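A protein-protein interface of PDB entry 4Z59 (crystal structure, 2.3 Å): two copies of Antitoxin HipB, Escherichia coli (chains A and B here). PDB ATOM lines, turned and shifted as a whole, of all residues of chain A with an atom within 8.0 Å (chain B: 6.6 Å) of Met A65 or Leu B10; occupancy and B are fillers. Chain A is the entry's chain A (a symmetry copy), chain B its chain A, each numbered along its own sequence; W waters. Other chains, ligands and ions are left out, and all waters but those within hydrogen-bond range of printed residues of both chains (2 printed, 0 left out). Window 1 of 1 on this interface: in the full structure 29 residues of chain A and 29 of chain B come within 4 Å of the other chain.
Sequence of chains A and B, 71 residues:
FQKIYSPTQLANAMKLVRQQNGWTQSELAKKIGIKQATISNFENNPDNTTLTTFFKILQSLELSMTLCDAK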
ATOM      1  N   ILE A   4      14.594 -21.607  16.310  1.00  0.00           N
ATOM      2  CA  ILE A   4      13.560 -22.620  16.092  1.00  0.00           C
ATOM      3  C   ILE A   4      13.920 -23.444  14.856  1.00  0.00           C
ATOM      4  O   ILE A   4      14.327 -22.885  13.829  1.00  0.00           O
ATOM      5  CB  ILE A   4      12.190 -21.918  15.935  1.00  0.00           C
ATOM      6  CG1 ILE A   4      11.774 -21.357  17.295  1.00  0.00           C
ATOM      7  CG2 ILE A   4      11.126 -22.868  15.349  1.00  0.00           C
ATOM      8  CD1 ILE A   4      10.670 -20.330  17.240  1.00  0.00           C
ATOM      9  N   LEU A  10       8.047 -24.475  16.348  1.00  0.00           N
ATOM     10  CA  LEU A  10       7.471 -23.193  15.980  1.00  0.00           C
ATOM     11  C   LEU A  10       6.070 -23.073  16.584  1.00  0.00           C
ATOM     12  O   LEU A  10       5.729 -22.047  17.190  1.00  0.00           O
ATOM     13  CB  LEU A  10       7.427 -23.045  14.461  1.00  0.00           C
ATOM     14  CG  LEU A  10       6.777 -21.758  13.935  1.00  0.00           C
ATOM     15  CD1 LEU A  10       7.582 -20.524  14.352  1.00  0.00           C
ATOM     16  CD2 LEU A  10       6.674 -21.833  12.411  1.00  0.00           C
ATOM     17  N   MET A  14       4.631 -20.370  19.279  1.00  0.00           N
ATOM     18  CA  MET A  14       3.550 -19.441  18.995  1.00  0.00           C
ATOM     19  C   MET A  14       2.325 -19.683  19.881  1.00  0.00           C
ATOM     20  O   MET A  14       1.623 -18.750  20.238  1.00  0.00           O
ATOM     21  CB  MET A  14       3.203 -19.448  17.502  1.00  0.00           C
ATOM     22  CG  MET A  14       4.329 -18.792  16.678  1.00  0.00           C
ATOM     23  SD  MET A  14       4.146 -19.054  14.911  1.00  0.00           S
ATOM     24  CE  MET A  14       2.679 -18.057  14.582  1.00  0.00           C
ATOM     25  N   LEU A  51       2.708 -21.922   4.624  1.00  0.00           N
ATOM     26  CA  LEU A  51       3.385 -20.685   5.006  1.00  0.00           C
ATOM     27  C   LEU A  51       2.420 -19.504   5.160  1.00  0.00           C
ATOM     28  O   LEU A  51       2.595 -18.656   6.042  1.00  0.00           O
ATOM     29  CB  LEU A  51       4.454 -20.334   3.988  1.00  0.00           C
ATOM     30  CG  LEU A  51       5.617 -21.299   4.007  1.00  0.00           C
ATOM     31  CD1 LEU A  51       6.593 -20.925   2.919  1.00  0.00           C
ATOM     32  CD2 LEU A  51       6.270 -21.251   5.381  1.00  0.00           C
ATOM     33  N   PHE A  54       0.864 -19.574   8.520  1.00  0.00           N
ATOM     34  CA  PHE A  54       1.896 -19.217   9.470  1.00  0.00           C
ATOM     35  C   PHE A  54       2.048 -17.685   9.551  1.00  0.00           C
ATOM     36  O   PHE A  54       2.025 -17.104  10.644  1.00  0.00           O
ATOM     37  CB  PHE A  54       3.221 -19.888   9.073  1.00  0.00           C
ATOM     38  CG  PHE A  54       4.424 -19.299   9.739  1.00  0.00           C
ATOM     39  CD1 PHE A  54       4.441 -19.071  11.111  1.00  0.00           C
ATOM     40  CD2 PHE A  54       5.562 -19.003   9.000  1.00  0.00           C
ATOM     41  CE1 PHE A  54       5.563 -18.525  11.729  1.00  0.00           C
ATOM     42  CE2 PHE A  54       6.699 -18.478   9.618  1.00  0.00           C
ATOM     43  CZ  PHE A  54       6.694 -18.229  10.984  1.00  0.00           C
ATOM     44  N   PHE A  55       2.179 -17.030   8.400  1.00  0.00           N
ATOM     45  CA  PHE A  55       2.364 -15.578   8.416  1.00  0.00           C
ATOM     46  C   PHE A  55       1.148 -14.801   8.875  1.00  0.00           C
ATOM     47  O   PHE A  55       1.294 -13.732   9.445  1.00  0.00           O
ATOM     48  CB  PHE A  55       2.922 -15.043   7.083  1.00  0.00           C
ATOM     49  CG  PHE A  55       4.395 -15.269   6.955  1.00  0.00           C
ATOM     50  CD1 PHE A  55       5.294 -14.456   7.651  1.00  0.00           C
ATOM     51  CD2 PHE A  55       4.881 -16.327   6.215  1.00  0.00           C
ATOM     52  CE1 PHE A  55       6.666 -14.678   7.585  1.00  0.00           C
ATOM     53  CE2 PHE A  55       6.259 -16.568   6.146  1.00  0.00           C
ATOM     54  CZ  PHE A  55       7.151 -15.749   6.835  1.00  0.00           C
ATOM     55  N   LEU A  58       1.128 -15.088  12.613  1.00  0.00           N
ATOM     56  CA  LEU A  58       2.178 -14.209  13.138  1.00  0.00           C
ATOM     57  C   LEU A  58       1.643 -12.803  13.295  1.00  0.00           C
ATOM     58  O   LEU A  58       1.887 -12.144  14.319  1.00  0.00           O
ATOM     59  CB  LEU A  58       3.377 -14.114  12.206  1.00  0.00           C
ATOM     60  CG  LEU A  58       4.536 -15.081  12.308  1.00  0.00           C
ATOM     61  CD1 LEU A  58       5.559 -14.694  11.255  1.00  0.00           C
ATOM     62  CD2 LEU A  58       5.181 -15.097  13.687  1.00  0.00           C
ATOM     63  N   LEU A  63       3.586 -10.504  15.844  1.00  0.00           N
ATOM     64  CA  LEU A  63       4.946 -10.984  15.652  1.00  0.00           C
ATOM     65  C   LEU A  63       5.422 -10.862  14.212  1.00  0.00           C
ATOM     66  O   LEU A  63       4.641 -10.715  13.281  1.00  0.00           O
ATOM     67  CB  LEU A  63       5.053 -12.447  16.072  1.00  0.00           C
ATOM     68  CG  LEU A  63       4.758 -12.750  17.533  1.00  0.00           C
ATOM     69  CD1 LEU A  63       4.756 -14.285  17.731  1.00  0.00           C
ATOM     70  CD2 LEU A  63       5.789 -12.048  18.451  1.00  0.00           C
ATOM     71  N   SER A  64       6.729 -10.953  14.051  1.00  0.00           N
ATOM     72  CA  SER A  64       7.349 -11.108  12.751  1.00  0.00           C
ATOM     73  C   SER A  64       8.359 -12.233  12.959  1.00  0.00           C
ATOM     74  O   SER A  64       8.387 -12.830  14.027  1.00  0.00           O
ATOM     75  CB  SER A  64       8.086  -9.820  12.411  1.00  0.00           C
ATOM     76  OG  SER A  64       8.722  -9.961  11.171  1.00  0.00           O
ATOM     77  N   MET A  65       9.227 -12.499  11.989  1.00  0.00           N
ATOM     78  CA  MET A  65      10.293 -13.475  12.203  1.00  0.00           C
ATOM     79  C   MET A  65      11.513 -13.028  11.434  1.00  0.00           C
ATOM     80  O   MET A  65      11.402 -12.176  10.560  1.00  0.00           O
ATOM     81  CB  MET A  65       9.868 -14.843  11.672  1.00  0.00           C
ATOM     82  CG  MET A  65       9.495 -14.787  10.201  1.00  0.00           C
ATOM     83  SD  MET A  65      10.140 -16.144   9.222  1.00  0.00           S
ATOM     84  CE  MET A  65      11.823 -15.703   9.045  1.00  0.00           C
ATOM     85  N   THR A  66      12.671 -13.596  11.754  1.00  0.00           N
ATOM     86  CA  THR A  66      13.888 -13.333  10.984  1.00  0.00           C
ATOM     87  C   THR A  66      14.641 -14.639  10.834  1.00  0.00           C
ATOM     88  O   THR A  66      14.466 -15.564  11.623  1.00  0.00           O
ATOM     89  CB  THR A  66      14.850 -12.303  11.667  1.00  0.00           C
ATOM     90  OG1 THR A  66      15.359 -12.849  12.887  1.00  0.00           O
ATOM     91  CG2 THR A  66      14.126 -11.038  12.017  1.00  0.00           C
ATOM     92  N   LEU A  67      15.467 -14.711   9.801  1.00  0.00           N
ATOM     93  CA  LEU A  67      16.374 -15.813   9.637  1.00  0.00           C
ATOM     94  C   LEU A  67      17.577 -15.581  10.541  1.00  0.00           C
ATOM     95  O   LEU A  67      17.833 -14.471  10.958  1.00  0.00           O
ATOM     96  CB  LEU A  67      16.855 -15.847   8.202  1.00  0.00           C
ATOM     97  CG  LEU A  67      15.720 -16.064   7.209  1.00  0.00           C
ATOM     98  CD1 LEU A  67      16.199 -15.776   5.782  1.00  0.00           C
ATOM     99  CD2 LEU A  67      15.208 -17.490   7.354  1.00  0.00           C
ATOM    100  N   CYS A  68      18.315 -16.637  10.838  1.00  0.00           N
ATOM    101  CA  CYS A  68      19.579 -16.486  11.518  1.00  0.00           C
ATOM    102  C   CYS A  68      20.390 -17.748  11.278  1.00  0.00           C
ATOM    103  O   CYS A  68      19.893 -18.715  10.687  1.00  0.00           O
ATOM    104  CB  CYS A  68      19.345 -16.285  13.012  1.00  0.00           C
ATOM    105  SG  CYS A  68      18.426 -17.624  13.731  1.00  0.00           S
ATOM    106  N   GLN B   2      16.708  -9.247   7.848  1.00  0.00           N
ATOM    107  CA  GLN B   2      15.613  -8.345   8.203  1.00  0.00           C
ATOM    108  C   GLN B   2      14.415  -9.127   8.741  1.00  0.00           C
ATOM    109  O   GLN B   2      14.316 -10.354   8.555  1.00  0.00           O
ATOM    110  CB  GLN B   2      15.135  -7.578   6.966  1.00  0.00           C
ATOM    111  CG  GLN B   2      16.211  -6.922   6.132  1.00  0.00           C
ATOM    112  CD  GLN B   2      16.710  -5.596   6.703  1.00  0.00           C
ATOM    113  OE1 GLN B   2      16.431  -5.239   7.860  1.00  0.00           O
ATOM    114  NE2 GLN B   2      17.457  -4.855   5.883  1.00  0.00           N
ATOM    115  N   LYS B   3      13.484  -8.411   9.365  1.00  0.00           N
ATOM    116  CA  LYS B   3      12.187  -8.985   9.704  1.00  0.00           C
ATOM    117  C   LYS B   3      11.410  -9.307   8.434  1.00  0.00           C
ATOM    118  O   LYS B   3      11.471  -8.560   7.452  1.00  0.00           O
ATOM    119  CB  LYS B   3      11.378  -8.028  10.569  1.00  0.00           C
ATOM    120  CG  LYS B   3      11.999  -7.801  11.928  1.00  0.00           C
ATOM    121  CD  LYS B   3      11.263  -6.748  12.674  1.00  0.00           C
ATOM    122  CE  LYS B   3      11.776  -6.655  14.093  1.00  0.00           C
ATOM    123  NZ  LYS B   3      10.839  -5.810  14.906  1.00  0.00           N
ATOM    124  N   ILE B   4      10.685 -10.424   8.471  1.00  0.00           N
ATOM    125  CA  ILE B   4       9.996 -10.982   7.307  1.00  0.00           C
ATOM    126  C   ILE B   4       8.520 -11.177   7.647  1.00  0.00           C
ATOM    127  O   ILE B   4       8.186 -11.667   8.735  1.00  0.00           O
ATOM    128  CB  ILE B   4      10.675 -12.315   6.909  1.00  0.00           C
ATOM    129  CG1 ILE B   4      12.050 -12.002   6.318  1.00  0.00           C
ATOM    130  CG2 ILE B   4       9.798 -13.134   5.940  1.00  0.00           C
ATOM    131  CD1 ILE B   4      12.982 -13.185   6.236  1.00  0.00           C
ATOM    132  N   TYR B   5       7.637 -10.791   6.736  1.00  0.00           N
ATOM    133  CA  TYR B   5       6.208 -10.733   7.057  1.00  0.00           C
ATOM    134  C   TYR B   5       5.310 -11.549   6.129  1.00  0.00           C
ATOM    135  O   TYR B   5       4.095 -11.530   6.287  1.00  0.00           O
ATOM    136  CB  TYR B   5       5.715  -9.274   7.028  1.00  0.00           C
ATOM    137  CG  TYR B   5       6.380  -8.391   8.049  1.00  0.00           C
ATOM    138  CD1 TYR B   5       7.636  -7.822   7.798  1.00  0.00           C
ATOM    139  CD2 TYR B   5       5.759  -8.113   9.255  1.00  0.00           C
ATOM    140  CE1 TYR B   5       8.250  -7.023   8.728  1.00  0.00           C
ATOM    141  CE2 TYR B   5       6.363  -7.303  10.195  1.00  0.00           C
ATOM    142  CZ  TYR B   5       7.615  -6.769   9.924  1.00  0.00           C
ATOM    143  OH  TYR B   5       8.227  -5.978  10.852  1.00  0.00           O
ATOM    144  N   SER B   6       5.875 -12.259   5.160  1.00  0.00           N
ATOM    145  CA  SER B   6       5.023 -12.939   4.181  1.00  0.00           C
ATOM    146  C   SER B   6       5.789 -14.083   3.528  1.00  0.00           C
ATOM    147  O   SER B   6       7.014 -14.089   3.534  1.00  0.00           O
ATOM    148  CB  SER B   6       4.594 -11.940   3.100  1.00  0.00           C
ATOM    149  OG  SER B   6       5.600 -11.853   2.098  1.00  0.00           O
ATOM    150  N   PRO B   7       5.080 -15.057   2.952  1.00  0.00           N
ATOM    151  CA  PRO B   7       5.833 -16.160   2.327  1.00  0.00           C
ATOM    152  C   PRO B   7       6.742 -15.670   1.180  1.00  0.00           C
ATOM    153  O   PRO B   7       7.875 -16.148   1.037  1.00  0.00           O
ATOM    154  CB  PRO B   7       4.725 -17.096   1.809  1.00  0.00           C
ATOM    155  CG  PRO B   7       3.536 -16.818   2.710  1.00  0.00           C
ATOM    156  CD  PRO B   7       3.629 -15.314   2.997  1.00  0.00           C
ATOM    157  N   THR B   8       6.266 -14.699   0.407  1.00  0.00           N
ATOM    158  CA  THR B   8       7.057 -14.122  -0.666  1.00  0.00           C
ATOM    159  C   THR B   8       8.353 -13.473  -0.159  1.00  0.00           C
ATOM    160  O   THR B   8       9.431 -13.684  -0.726  1.00  0.00           O
ATOM    161  CB  THR B   8       6.228 -13.118  -1.472  1.00  0.00           C
ATOM    162  OG1 THR B   8       5.125 -13.817  -2.053  1.00  0.00           O
ATOM    163  CG2 THR B   8       7.074 -12.490  -2.594  1.00  0.00           C
ATOM    164  N   GLN B   9       8.278 -12.716   0.928  1.00  0.00           N
ATOM    165  CA  GLN B   9       9.503 -12.135   1.456  1.00  0.00           C
ATOM    166  C   GLN B   9      10.432 -13.228   1.965  1.00  0.00           C
ATOM    167  O   GLN B   9      11.651 -13.124   1.865  1.00  0.00           O
ATOM    168  CB  GLN B   9       9.189 -11.147   2.580  1.00  0.00           C
ATOM    169  CG  GLN B   9       8.337  -9.983   2.136  1.00  0.00           C
ATOM    170  CD  GLN B   9       8.008  -9.045   3.305  1.00  0.00           C
ATOM    171  OE1 GLN B   9       8.480  -9.249   4.429  1.00  0.00           O
ATOM    172  NE2 GLN B   9       7.202  -8.017   3.037  1.00  0.00           N
ATOM    173  N   LEU B  10       9.852 -14.285   2.515  1.00  0.00           N
ATOM    174  CA  LEU B  10      10.669 -15.347   3.075  1.00  0.00           C
ATOM    175  C   LEU B  10      11.417 -16.063   1.949  1.00  0.00           C
ATOM    176  O   LEU B  10      12.630 -16.292   2.043  1.00  0.00           O
ATOM    177  CB  LEU B  10       9.800 -16.326   3.864  1.00  0.00           C
ATOM    178  CG  LEU B  10      10.532 -17.540   4.455  1.00  0.00           C
ATOM    179  CD1 LEU B  10      11.559 -17.104   5.506  1.00  0.00           C
ATOM    180  CD2 LEU B  10       9.510 -18.491   5.076  1.00  0.00           C
ATOM    181  N   ALA B  11      10.689 -16.399   0.882  1.00  0.00           N
ATOM    182  CA  ALA B  11      11.275 -17.109  -0.250  1.00  0.00           C
ATOM    183  C   ALA B  11      12.349 -16.243  -0.915  1.00  0.00           C
ATOM    184  O   ALA B  11      13.438 -16.717  -1.184  1.00  0.00           O
ATOM    185  CB  ALA B  11      10.182 -17.529  -1.269  1.00  0.00           C
ATOM    186  N   ASN B  12      12.060 -14.965  -1.136  1.00  0.00           N
ATOM    187  CA  ASN B  12      13.095 -14.079  -1.659  1.00  0.00           C
ATOM    188  C   ASN B  12      14.345 -14.062  -0.768  1.00  0.00           C
ATOM    189  O   ASN B  12      15.463 -14.204  -1.277  1.00  0.00           O
ATOM    190  CB  ASN B  12      12.564 -12.670  -1.929  1.00  0.00           C
ATOM    191  CG  ASN B  12      11.394 -12.667  -2.920  1.00  0.00           C
ATOM    192  OD1 ASN B  12      11.168 -13.640  -3.660  1.00  0.00           O
ATOM    193  ND2 ASN B  12      10.634 -11.584  -2.919  1.00  0.00           N
ATOM    194  N   ALA B  13      14.163 -13.966   0.551  1.00  0.00           N
ATOM    195  CA  ALA B  13      15.320 -13.996   1.454  1.00  0.00           C
ATOM    196  C   ALA B  13      16.121 -15.285   1.357  1.00  0.00           C
ATOM    197  O   ALA B  13      17.347 -15.254   1.306  1.00  0.00           O
ATOM    198  CB  ALA B  13      14.916 -13.754   2.894  1.00  0.00           C
ATOM    199  N   MET B  14      15.431 -16.417   1.318  1.00  0.00           N
ATOM    200  CA  MET B  14      16.138 -17.687   1.304  1.00  0.00           C
ATOM    201  C   MET B  14      16.770 -17.987  -0.060  1.00  0.00           C
ATOM    202  O   MET B  14      17.823 -18.599  -0.135  1.00  0.00           O
ATOM    203  CB  MET B  14      15.232 -18.822   1.791  1.00  0.00           C
ATOM    204  CG  MET B  14      14.966 -18.695   3.304  1.00  0.00           C
ATOM    205  SD  MET B  14      13.663 -19.788   3.880  1.00  0.00           S
ATOM    206  CE  MET B  14      14.465 -21.390   3.676  1.00  0.00           C
ATOM    207  N   LYS B  15      16.146 -17.536  -1.139  1.00  0.00           N
ATOM    208  CA  LYS B  15      16.764 -17.723  -2.441  1.00  0.00           C
ATOM    209  C   LYS B  15      18.084 -16.938  -2.527  1.00  0.00           C
ATOM    210  O   LYS B  15      19.110 -17.438  -3.008  1.00  0.00           O
ATOM    211  CB  LYS B  15      15.816 -17.299  -3.546  1.00  0.00           C
ATOM    212  CG  LYS B  15      16.475 -17.337  -4.922  1.00  0.00           C
ATOM    213  CD  LYS B  15      15.458 -17.052  -6.002  1.00  0.00           C
ATOM    214  CE  LYS B  15      16.107 -17.082  -7.388  1.00  0.00           C
ATOM    215  NZ  LYS B  15      15.079 -16.842  -8.438  1.00  0.00           N
ATOM    216  N   PHE B  42       8.799 -23.636  -3.928  1.00  0.00           N
ATOM    217  CA  PHE B  42       8.959 -22.768  -2.774  1.00  0.00           C
ATOM    218  C   PHE B  42       9.536 -21.397  -3.156  1.00  0.00           C
ATOM    219  O   PHE B  42       8.985 -20.367  -2.785  1.00  0.00           O
ATOM    220  CB  PHE B  42       9.848 -23.412  -1.699  1.00  0.00           C
ATOM    221  CG  PHE B  42      10.358 -22.423  -0.672  1.00  0.00           C
ATOM    222  CD1 PHE B  42       9.475 -21.797   0.207  1.00  0.00           C
ATOM    223  CD2 PHE B  42      11.712 -22.104  -0.598  1.00  0.00           C
ATOM    224  CE1 PHE B  42       9.922 -20.897   1.154  1.00  0.00           C
ATOM    225  CE2 PHE B  42      12.181 -21.194   0.366  1.00  0.00           C
ATOM    226  CZ  PHE B  42      11.284 -20.586   1.236  1.00  0.00           C
ATOM    227  N   PRO B  46       5.637 -19.599  -2.904  1.00  0.00           N
ATOM    228  CA  PRO B  46       5.709 -20.099  -1.520  1.00  0.00           C
ATOM    229  C   PRO B  46       4.409 -20.112  -0.702  1.00  0.00           C
ATOM    230  O   PRO B  46       4.429 -20.695   0.380  1.00  0.00           O
ATOM    231  CB  PRO B  46       6.683 -19.137  -0.853  1.00  0.00           C
ATOM    232  CG  PRO B  46       6.494 -17.842  -1.625  1.00  0.00           C
ATOM    233  CD  PRO B  46       6.323 -18.298  -3.052  1.00  0.00           C
ATOM    234  N   PHE B  54       9.765 -25.812   4.513  1.00  0.00           N
ATOM    235  CA  PHE B  54      10.446 -24.609   4.937  1.00  0.00           C
ATOM    236  C   PHE B  54      11.598 -24.951   5.902  1.00  0.00           C
ATOM    237  O   PHE B  54      12.740 -24.514   5.705  1.00  0.00           O
ATOM    238  CB  PHE B  54       9.440 -23.647   5.589  1.00  0.00           C
ATOM    239  CG  PHE B  54      10.075 -22.560   6.397  1.00  0.00           C
ATOM    240  CD1 PHE B  54      11.129 -21.811   5.885  1.00  0.00           C
ATOM    241  CD2 PHE B  54       9.596 -22.254   7.665  1.00  0.00           C
ATOM    242  CE1 PHE B  54      11.718 -20.798   6.638  1.00  0.00           C
ATOM    243  CE2 PHE B  54      10.166 -21.224   8.415  1.00  0.00           C
ATOM    244  CZ  PHE B  54      11.236 -20.502   7.903  1.00  0.00           C
ATOM    245  N   LEU B  58      15.673 -24.671   5.370  1.00  0.00           N
ATOM    246  CA  LEU B  58      16.460 -23.876   6.318  1.00  0.00           C
ATOM    247  C   LEU B  58      17.700 -24.640   6.727  1.00  0.00           C
ATOM    248  O   LEU B  58      18.803 -24.070   6.782  1.00  0.00           O
ATOM    249  CB  LEU B  58      15.697 -23.574   7.598  1.00  0.00           C
ATOM    250  CG  LEU B  58      14.827 -22.343   7.729  1.00  0.00           C
ATOM    251  CD1 LEU B  58      14.233 -22.338   9.126  1.00  0.00           C
ATOM    252  CD2 LEU B  58      15.586 -21.048   7.476  1.00  0.00           C
ATOM    253  N   SER B  64      18.579 -21.052  10.754  1.00  0.00           N
ATOM    254  CA  SER B  64      17.503 -21.313  11.688  1.00  0.00           C
ATOM    255  C   SER B  64      16.616 -20.075  11.578  1.00  0.00           C
ATOM    256  O   SER B  64      16.863 -19.228  10.730  1.00  0.00           O
ATOM    257  CB  SER B  64      18.091 -21.393  13.091  1.00  0.00           C
ATOM    258  OG  SER B  64      17.062 -21.612  14.014  1.00  0.00           O
ATOM    259  N   MET B  65      15.626 -19.923  12.450  1.00  0.00           N
ATOM    260  CA  MET B  65      14.841 -18.691  12.461  1.00  0.00           C
ATOM    261  C   MET B  65      14.438 -18.392  13.885  1.00  0.00           C
ATOM    262  O   MET B  65      14.520 -19.271  14.737  1.00  0.00           O
ATOM    263  CB  MET B  65      13.569 -18.868  11.631  1.00  0.00           C
ATOM    264  CG  MET B  65      12.728 -20.031  12.130  1.00  0.00           C
ATOM    265  SD  MET B  65      10.970 -19.688  12.216  1.00  0.00           S
ATOM    266  CE  MET B  65      10.858 -18.698  13.653  1.00  0.00           C
ATOM    267  N   THR B  66      14.004 -17.162  14.146  1.00  0.00           N
ATOM    268  CA  THR B  66      13.465 -16.808  15.461  1.00  0.00           C
ATOM    269  C   THR B  66      12.261 -15.913  15.250  1.00  0.00           C
ATOM    270  O   THR B  66      12.125 -15.270  14.210  1.00  0.00           O
ATOM    271  CB  THR B  66      14.482 -16.034  16.366  1.00  0.00           C
ATOM    272  OG1 THR B  66      14.774 -14.759  15.786  1.00  0.00           O
ATOM    273  CG2 THR B  66      15.781 -16.775  16.476  1.00  0.00           C
ATOM    274  N   LEU B  67      11.381 -15.891  16.237  1.00  0.00           N
ATOM    275  CA  LEU B  67      10.289 -14.957  16.253  1.00  0.00           C
ATOM    276  C   LEU B  67      10.815 -13.613  16.736  1.00  0.00           C
ATOM    277  O   LEU B  67      11.854 -13.543  17.359  1.00  0.00           O
ATOM    278  CB  LEU B  67       9.240 -15.441  17.234  1.00  0.00           C
ATOM    279  CG  LEU B  67       8.656 -16.791  16.847  1.00  0.00           C
ATOM    280  CD1 LEU B  67       7.849 -17.377  18.012  1.00  0.00           C
ATOM    281  CD2 LEU B  67       7.796 -16.616  15.603  1.00  0.00           C
ATOM    282  N   CYS B  68      10.088 -12.548  16.448  1.00  0.00           N
ATOM    283  CA  CYS B  68      10.397 -11.263  17.030  1.00  0.00           C
ATOM    284  C   CYS B  68       9.158 -10.394  16.925  1.00  0.00           C
ATOM    285  O   CYS B  68       8.156 -10.792  16.316  1.00  0.00           O
ATOM    286  CB  CYS B  68      11.558 -10.619  16.280  1.00  0.00           C
ATOM    287  SG  CYS B  68      11.214 -10.432  14.548  1.00  0.00           S
ATOM    288  N   ASP B  69       9.216  -9.205  17.516  1.00  0.00           N
ATOM    289  CA  ASP B  69       8.048  -8.328  17.526  1.00  0.00           C
ATOM    290  C   ASP B  69       7.781  -7.797  16.138  1.00  0.00           C
ATOM    291  O   ASP B  69       8.711  -7.565  15.370  1.00  0.00           O
ATOM    292  CB  ASP B  69       8.230  -7.203  18.540  1.00  0.00           C
ATOM    293  CG  ASP B  69       8.526  -7.746  19.937  1.00  0.00           C
ATOM    294  OD1 ASP B  69       7.824  -8.690  20.383  1.00  0.00           O
ATOM    295  OD2 ASP B  69       9.481  -7.259  20.580  1.00  0.00           O
HETATM  296  O   HOH W   1      15.680 -12.581   7.999  1.00  0.00           O
HETATM  297  O   HOH W   2       3.160 -11.722   9.061  1.00  0.00           O
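The backbone NH of Thr B66 sits at hydrogen-bond distance from the backbone carbonyl oxygen of Thr A66, 3.0 Å away. O of Cys A68 sits at hydrogen-bond distance from N of Ser B64 (2.7 Å). The backbone NH (N) of Ile B4 is in hydrogen-bond range of the backbone carbonyl oxygen (O) of Met A65, at 2.8 Å. The side-chain hydroxyl of Ser A64 sits at hydrogen-bond distance from the backbone carbonyl oxygen of Ile B4 (3.0 Å). N of Ile A4 is in hydrogen-bond range of O of Met B65. The backbone carbonyl oxygen of Cys B68 lies within hydrogen-bond range of the backbone NH of Ser A64. OG of Ser B64 sits at hydrogen-bond distance from O of Ile A4 (3.0 Å).
The backbone NH (N) of Gln B9 is in hydrogen-bond range of the side-chain hydroxyl (OG) of Ser B6, at 3.0 Å. The backbone carbonyl oxygen (O) of Leu A58 is in hydrogen-bond range of the backbone NH (N) of Leu A63, 2.8 Å away. The side-chain amide oxygen (OE1) of Gln B9 lies within hydrogen-bond range of the backbone NH (N) of Tyr B5 (2.9 Å). N of Thr B8 lies close to OG of Ser B6, 3.4 Å away. NZ of Lys B3 lies within hydrogen-bond range of O of Asp B69 (2.8 Å).
Leu A51 touches Phe B42 (CD1 to CE1, 3.8 Å). Leu A51 touches Phe B54 (CD2 to CB, 3.98 Å). Ile B4 touches Phe A55. CD1 of Phe A55 touches C of Tyr B5, at 3.3 Å. Pro B7 touches Phe A55 (N to CD2, 3.5 Å). Leu A63 touches Cys B68 (CA to O, 3.3 Å). Lys B3 touches Ser A64. Tyr B5 touches Ser A64. Thr A66 touches Lys B3 (CG2 to CA, 3.7 Å). Thr A66 touches Met B65 (O to CA, 3.3 Å).
Printed residues of chain B within 4 Å of Ser A64: Lys B3, Ile B4, Tyr B5, Leu B67, Cys B68 and Asp B69. Of chain B, only Gln B2 (3.98 Å), Lys B3 (3.4 Å), Ile B4 (2.8 Å), Leu B10 (3.8 Å), Thr B66 (3.3 Å) and Cys B68 (3.8 Å) come within 4 Å of Met A65. Of the printed residues of chain B, Leu A67 touches Ala B13 (3.8 Å), Leu B58 (3.6 Å) and Ser B64 (3.6 Å). Of chain A, only Phe A55 (3.9 Å) and Met A65 (3.8 Å) come within 4 Å of Leu B10. No residue of chain A comes within 4 Å of Ala B11. Met B14 touches none of the printed residues of chain A. Of the printed residues of chain A, Leu B67 touches Leu A58 and Ser A64. Printed residues of chain A within 4 Å of Cys B68: Leu A63 (3.3 Å), Ser A64 (2.7 Å), Met A65 (3.8 Å) and Thr A66 (3.9 Å).
Hydrophobic or aromatic side chains of chain B that line the printed part of chain A: Ile B4, Tyr B5, Pro B7, Leu B10, Ala B13, Phe B42, Phe B54, Leu B58, Met B65 and Leu B67. Hydrophobic or aromatic side chains of chain A within 4 Å of the printed part of chain B: Ile A4, Leu A10, Leu A51, Phe A55, Leu A58, Leu A63, Met A65 and Leu A67. Among the printed residues, 37 pairs touch across the chains. Among the printed residues, no Asp or Glu carboxylate lies within 4 Å of a Lys or Arg side-chain nitrogen of the other chain.
Leu A10 touches Met B65, and with the chains exchanged Met A65 touches Leu B10. Met A65 touches Cys B68, and with the chains exchanged Cys A68 touches Met B65. Thr A66 touches its own counterpart, Thr B66. Thr A66 touches Cys B68, and with the chains exchanged Cys A68 touches Thr B66.
Water W1 lies within hydrogen-bond range of O of Gln B2 (2.7 Å) and N of Leu A67 (2.8 Å). Water W2 lies within hydrogen-bond range of O of Phe A55 (2.8 Å) and O of Tyr B5 (2.9 Å).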
